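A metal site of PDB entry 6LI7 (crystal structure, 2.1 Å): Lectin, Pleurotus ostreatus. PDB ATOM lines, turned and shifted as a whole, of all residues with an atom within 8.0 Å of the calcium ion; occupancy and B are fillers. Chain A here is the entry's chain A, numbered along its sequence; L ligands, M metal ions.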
ATOM      1  N   TRP A  57      -8.383  -2.502  13.675  1.00  0.00           N
ATOM      2  CA  TRP A  57      -8.079  -2.375  12.245  1.00  0.00           C
ATOM      3  C   TRP A  57      -6.945  -3.359  11.972  1.00  0.00           C
ATOM      4  O   TRP A  57      -6.803  -4.293  12.777  1.00  0.00           O
ATOM      5  CB  TRP A  57      -7.743  -0.901  11.930  1.00  0.00           C
ATOM      6  CG  TRP A  57      -7.754  -0.606  10.477  1.00  0.00           C
ATOM      7  CD1 TRP A  57      -6.690  -0.253   9.694  1.00  0.00           C
ATOM      8  CD2 TRP A  57      -8.904  -0.613   9.603  1.00  0.00           C
ATOM      9  NE1 TRP A  57      -7.091  -0.062   8.411  1.00  0.00           N
ATOM     10  CE2 TRP A  57      -8.438  -0.276   8.309  1.00  0.00           C
ATOM     11  CE3 TRP A  57     -10.271  -0.850   9.803  1.00  0.00           C
ATOM     12  CZ2 TRP A  57      -9.302  -0.189   7.215  1.00  0.00           C
ATOM     13  CZ3 TRP A  57     -11.138  -0.723   8.725  1.00  0.00           C
ATOM     14  CH2 TRP A  57     -10.638  -0.422   7.447  1.00  0.00           C
ATOM     15  N   GLY A  66      -3.761   6.141  14.086  1.00  0.00           N
ATOM     16  CA  GLY A  66      -2.882   6.810  13.124  1.00  0.00           C
ATOM     17  C   GLY A  66      -3.512   6.902  11.740  1.00  0.00           C
ATOM     18  O   GLY A  66      -4.649   6.339  11.537  1.00  0.00           O
ATOM     19  N   ASN A  68      -4.277   6.010   7.939  1.00  0.00           N
ATOM     20  CA  ASN A  68      -4.473   4.797   7.165  1.00  0.00           C
ATOM     21  C   ASN A  68      -4.884   5.241   5.758  1.00  0.00           C
ATOM     22  O   ASN A  68      -5.426   6.354   5.593  1.00  0.00           O
ATOM     23  CB  ASN A  68      -5.451   3.845   7.850  1.00  0.00           C
ATOM     24  CG  ASN A  68      -4.800   3.165   9.046  1.00  0.00           C
ATOM     25  OD1 ASN A  68      -4.829   3.682  10.177  1.00  0.00           O
ATOM     26  ND2 ASN A  68      -4.280   1.997   8.812  1.00  0.00           N
ATOM     27  N   ILE A  69      -4.565   4.395   4.802  1.00  0.00           N
ATOM     28  CA  ILE A  69      -4.926   4.593   3.366  1.00  0.00           C
ATOM     29  C   ILE A  69      -6.419   4.285   3.203  1.00  0.00           C
ATOM     30  O   ILE A  69      -6.993   3.546   4.045  1.00  0.00           O
ATOM     31  CB  ILE A  69      -4.069   3.705   2.452  1.00  0.00           C
ATOM     32  CG1 ILE A  69      -4.346   2.219   2.683  1.00  0.00           C
ATOM     33  CG2 ILE A  69      -2.574   4.061   2.595  1.00  0.00           C
ATOM     34  CD1 ILE A  69      -3.699   1.292   1.655  1.00  0.00           C
ATOM     35  N   ILE A  70      -6.975   4.755   2.103  1.00  0.00           N
ATOM     36  CA  ILE A  70      -8.321   4.345   1.628  1.00  0.00           C
ATOM     37  C   ILE A  70      -8.224   2.861   1.331  1.00  0.00           C
ATOM     38  O   ILE A  70      -7.335   2.461   0.653  1.00  0.00           O
ATOM     39  CB  ILE A  70      -8.769   5.181   0.415  1.00  0.00           C
ATOM     40  CG1 ILE A  70      -8.996   6.628   0.847  1.00  0.00           C
ATOM     41  CG2 ILE A  70     -10.004   4.546  -0.198  1.00  0.00           C
ATOM     42  CD1 ILE A  70      -9.260   7.576  -0.287  1.00  0.00           C
ATOM     43  N   SER A  96     -18.183   2.450  13.146  1.00  0.00           N
ATOM     44  CA  SER A  96     -17.102   2.318  12.148  1.00  0.00           C
ATOM     45  C   SER A  96     -16.577   3.685  11.758  1.00  0.00           C
ATOM     46  O   SER A  96     -17.336   4.636  11.623  1.00  0.00           O
ATOM     47  CB  SER A  96     -17.543   1.541  10.921  1.00  0.00           C
ATOM     48  OG  SER A  96     -18.652   2.176  10.266  1.00  0.00           O
ATOM     49  N   ASP A  97     -15.289   3.729  11.562  1.00  0.00           N
ATOM     50  CA  ASP A  97     -14.609   4.825  10.860  1.00  0.00           C
ATOM     51  C   ASP A  97     -13.986   4.140   9.642  1.00  0.00           C
ATOM     52  O   ASP A  97     -12.953   3.506   9.810  1.00  0.00           O
ATOM     53  CB  ASP A  97     -13.580   5.524  11.751  1.00  0.00           C
ATOM     54  CG  ASP A  97     -12.851   6.640  11.032  1.00  0.00           C
ATOM     55  OD1 ASP A  97     -12.955   6.699   9.772  1.00  0.00           O
ATOM     56  OD2 ASP A  97     -12.244   7.478  11.716  1.00  0.00           O
ATOM     57  N   ASP A  98     -14.594   4.260   8.431  1.00  0.00           N
ATOM     58  CA  ASP A  98     -15.718   5.116   8.087  1.00  0.00           C
ATOM     59  C   ASP A  98     -16.999   4.320   7.860  1.00  0.00           C
ATOM     60  O   ASP A  98     -18.082   4.876   8.010  1.00  0.00           O
ATOM     61  CB  ASP A  98     -15.426   5.861   6.778  1.00  0.00           C
ATOM     62  CG  ASP A  98     -14.342   6.909   6.918  1.00  0.00           C
ATOM     63  OD1 ASP A  98     -14.670   8.016   7.331  1.00  0.00           O
ATOM     64  OD2 ASP A  98     -13.154   6.595   6.618  1.00  0.00           O
ATOM     65  N   ALA A  99     -16.920   3.049   7.457  1.00  0.00           N
ATOM     66  CA  ALA A  99     -18.152   2.319   7.086  1.00  0.00           C
ATOM     67  C   ALA A  99     -17.960   0.816   7.303  1.00  0.00           C
ATOM     68  O   ALA A  99     -16.804   0.362   7.324  1.00  0.00           O
ATOM     69  CB  ALA A  99     -18.515   2.651   5.642  1.00  0.00           C
ATOM     70  N   PHE A 115     -18.920   6.846  13.580  1.00  0.00           N
ATOM     71  CA  PHE A 115     -18.309   6.486  14.884  1.00  0.00           C
ATOM     72  C   PHE A 115     -18.934   7.290  16.023  1.00  0.00           C
ATOM     73  O   PHE A 115     -18.726   6.907  17.177  1.00  0.00           O
ATOM     74  CB  PHE A 115     -16.801   6.676  14.804  1.00  0.00           C
ATOM     75  CG  PHE A 115     -16.329   8.062  14.448  1.00  0.00           C
ATOM     76  CD1 PHE A 115     -16.155   9.009  15.443  1.00  0.00           C
ATOM     77  CD2 PHE A 115     -15.947   8.360  13.139  1.00  0.00           C
ATOM     78  CE1 PHE A 115     -15.661  10.268  15.119  1.00  0.00           C
ATOM     79  CE2 PHE A 115     -15.486   9.630  12.801  1.00  0.00           C
ATOM     80  CZ  PHE A 115     -15.382  10.588  13.793  1.00  0.00           C
ATOM     81  N   GLN A 137     -14.320  -0.155   5.967  1.00  0.00           N
ATOM     82  CA  GLN A 137     -13.760   0.670   4.882  1.00  0.00           C
ATOM     83  C   GLN A 137     -13.285   1.971   5.485  1.00  0.00           C
ATOM     84  O   GLN A 137     -14.080   2.650   6.160  1.00  0.00           O
ATOM     85  CB  GLN A 137     -14.754   1.046   3.757  1.00  0.00           C
ATOM     86  CG  GLN A 137     -15.456  -0.159   3.138  1.00  0.00           C
ATOM     87  CD  GLN A 137     -16.672   0.277   2.332  1.00  0.00           C
ATOM     88  OE1 GLN A 137     -16.575   1.228   1.567  1.00  0.00           O
ATOM     89  NE2 GLN A 137     -17.825  -0.350   2.565  1.00  0.00           N
ATOM     90  N   ASN A 138     -12.062   2.330   5.171  1.00  0.00           N
ATOM     91  CA  ASN A 138     -11.550   3.697   5.391  1.00  0.00           C
ATOM     92  C   ASN A 138     -11.768   4.466   4.090  1.00  0.00           C
ATOM     93  O   ASN A 138     -11.271   3.999   3.023  1.00  0.00           O
ATOM     94  CB  ASN A 138     -10.075   3.655   5.722  1.00  0.00           C
ATOM     95  CG  ASN A 138      -9.576   4.982   6.196  1.00  0.00           C
ATOM     96  OD1 ASN A 138     -10.372   5.769   6.743  1.00  0.00           O
ATOM     97  ND2 ASN A 138      -8.273   5.206   6.032  1.00  0.00           N
ATOM     98  N   LEU A 139     -12.463   5.599   4.173  1.00  0.00           N
ATOM     99  CA  LEU A 139     -12.921   6.316   2.966  1.00  0.00           C
ATOM    100  C   LEU A 139     -12.200   7.643   2.832  1.00  0.00           C
ATOM    101  O   LEU A 139     -12.368   8.224   1.820  1.00  0.00           O
ATOM    102  CB  LEU A 139     -14.441   6.519   2.991  1.00  0.00           C
ATOM    103  CG  LEU A 139     -15.254   5.231   2.869  1.00  0.00           C
ATOM    104  CD1 LEU A 139     -16.743   5.516   2.997  1.00  0.00           C
ATOM    105  CD2 LEU A 139     -14.950   4.510   1.565  1.00  0.00           C
ATOM    106  N   VAL A 140     -11.406   8.093   3.811  1.00  0.00           N
ATOM    107  CA  VAL A 140     -10.657   9.368   3.696  1.00  0.00           C
ATOM    108  C   VAL A 140      -9.170   9.065   3.828  1.00  0.00           C
ATOM    109  O   VAL A 140      -8.764   8.364   4.825  1.00  0.00           O
ATOM    110  CB  VAL A 140     -11.148  10.342   4.770  1.00  0.00           C
ATOM    111  CG1 VAL A 140     -10.360  11.628   4.745  1.00  0.00           C
ATOM    112  CG2 VAL A 140     -12.636  10.613   4.605  1.00  0.00           C
ATOM    113  N   ALA A 141      -8.366   9.534   2.885  1.00  0.00           N
ATOM    114  CA  ALA A 141      -6.905   9.303   2.861  1.00  0.00           C
ATOM    115  C   ALA A 141      -6.250   9.969   4.083  1.00  0.00           C
ATOM    116  O   ALA A 141      -6.761  10.985   4.566  1.00  0.00           O
ATOM    117  CB  ALA A 141      -6.315   9.830   1.578  1.00  0.00           C
ATOM    118  N   ASN A 142      -5.213   9.345   4.624  1.00  0.00           N
ATOM    119  CA  ASN A 142      -4.435   9.848   5.782  1.00  0.00           C
ATOM    120  C   ASN A 142      -5.310   9.975   7.048  1.00  0.00           C
ATOM    121  O   ASN A 142      -4.926  10.755   7.914  1.00  0.00           O
ATOM    122  CB  ASN A 142      -3.850  11.227   5.536  1.00  0.00           C
ATOM    123  CG  ASN A 142      -3.011  11.231   4.300  1.00  0.00           C
ATOM    124  OD1 ASN A 142      -2.211  10.332   4.141  1.00  0.00           O
ATOM    125  ND2 ASN A 142      -3.290  12.157   3.397  1.00  0.00           N
ATOM    126  N   SER A 143      -6.397   9.208   7.170  1.00  0.00           N
ATOM    127  CA  SER A 143      -7.333   9.371   8.287  1.00  0.00           C
ATOM    128  C   SER A 143      -7.331   8.089   9.104  1.00  0.00           C
ATOM    129  O   SER A 143      -7.017   6.995   8.622  1.00  0.00           O
ATOM    130  CB  SER A 143      -8.742   9.721   7.772  1.00  0.00           C
ATOM    131  OG  SER A 143      -9.360   8.549   7.255  1.00  0.00           O
ATOM    132  N   PRO A 144      -7.739   8.153  10.375  1.00  0.00           N
ATOM    133  CA  PRO A 144      -7.852   6.934  11.168  1.00  0.00           C
ATOM    134  C   PRO A 144      -8.852   5.955  10.558  1.00  0.00           C
ATOM    135  O   PRO A 144      -9.733   6.370   9.811  1.00  0.00           O
ATOM    136  CB  PRO A 144      -8.381   7.394  12.533  1.00  0.00           C
ATOM    137  CG  PRO A 144      -8.397   8.867  12.512  1.00  0.00           C
ATOM    138  CD  PRO A 144      -8.092   9.362  11.104  1.00  0.00           C
ATOM    139  N   ALA A 145      -8.756   4.687  10.963  1.00  0.00           N
ATOM    140  CA  ALA A 145      -9.690   3.613  10.553  1.00  0.00           C
ATOM    141  C   ALA A 145      -9.930   2.664  11.735  1.00  0.00           C
ATOM    142  O   ALA A 145      -8.953   2.344  12.492  1.00  0.00           O
ATOM    143  CB  ALA A 145      -9.133   2.908   9.350  1.00  0.00           C
ATOM    144  N   GLY A 146     -11.172   2.215  11.877  1.00  0.00           N
ATOM    145  CA  GLY A 146     -11.503   1.246  12.926  1.00  0.00           C
ATOM    146  C   GLY A 146     -12.938   0.787  12.911  1.00  0.00           C
ATOM    147  O   GLY A 146     -13.864   1.517  12.431  1.00  0.00           O
ATOM    148  N   TRP A 204     -11.565   8.437  18.755  1.00  0.00           N
ATOM    149  CA  TRP A 204     -12.998   8.603  18.395  1.00  0.00           C
ATOM    150  C   TRP A 204     -13.801   9.105  19.593  1.00  0.00           C
ATOM    151  O   TRP A 204     -14.823   9.763  19.387  1.00  0.00           O
ATOM    152  CB  TRP A 204     -13.537   7.278  17.835  1.00  0.00           C
ATOM    153  CG  TRP A 204     -12.878   6.944  16.561  1.00  0.00           C
ATOM    154  CD1 TRP A 204     -13.007   7.583  15.346  1.00  0.00           C
ATOM    155  CD2 TRP A 204     -11.885   5.940  16.378  1.00  0.00           C
ATOM    156  NE1 TRP A 204     -12.173   7.003  14.428  1.00  0.00           N
ATOM    157  CE2 TRP A 204     -11.482   5.983  15.037  1.00  0.00           C
ATOM    158  CE3 TRP A 204     -11.297   5.003  17.242  1.00  0.00           C
ATOM    159  CZ2 TRP A 204     -10.498   5.139  14.531  1.00  0.00           C
ATOM    160  CZ3 TRP A 204     -10.315   4.196  16.739  1.00  0.00           C
ATOM    161  CH2 TRP A 204      -9.945   4.239  15.393  1.00  0.00           C
HETATM  162  C1  LIG L   1     -11.887  11.146  10.906  1.00  0.00           C
HETATM  163  O1  LIG L   1     -12.756  12.253  10.707  1.00  0.00           O
HETATM  164  C2  LIG L   1     -12.223  10.008   9.966  1.00  0.00           C
HETATM  165  O2  LIG L   1     -11.163   9.044   9.917  1.00  0.00           O
HETATM  166  C3  LIG L   1     -12.572  10.461   8.567  1.00  0.00           C
HETATM  167  O3  LIG L   1     -12.462   9.384   7.643  1.00  0.00           O
HETATM  168 CA    CA M   1     -11.302   7.291   8.272  1.00  0.00          CA
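The calcium ion is bound by OD1 of Asp 97 (2.3 Å), OD1 of Asn 138 (2.3 Å), O of Pro 144 (2.4 Å), O2 of the ligand (2.4 Å), O3 of the ligand (2.5 Å), OG of Ser 143 (2.5 Å) and OD2 of Asp 98 (2.6 Å).
The backbone carbonyl oxygen of Ser 143 lies within hydrogen-bond range of the backbone NH of Asn 68, at 3.0 Å.
The side-chain amide nitrogen of Asn 138 is in hydrogen-bond range of the backbone carbonyl oxygen of Ile 69 (2.9 Å).
ND2 of Asn 138 lies within hydrogen-bond range of O of Val 140 (3.4 Å).
The backbone NH (N) of Leu 139 sits close to the side-chain carboxylate (OD2) of Asp 98 (2.7 Å).
OG of Ser 143 sits close to O of Val 140 (2.5 Å).
O of Gln 137 sits at hydrogen-bond distance from N of Asp 98 (2.8 Å).
The indole nitrogen of Trp 204 lies within hydrogen-bond range of the side-chain carboxylate of Asp 97.
The backbone carbonyl oxygen (O) of Asn 68 is in hydrogen-bond range of the side-chain amide nitrogen (ND2) of Asn 138, 3.1 Å away.
Within 4 Å of the calcium ion: Asp 97, Asp 98, Asn 138, Ser 143 and Pro 144.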
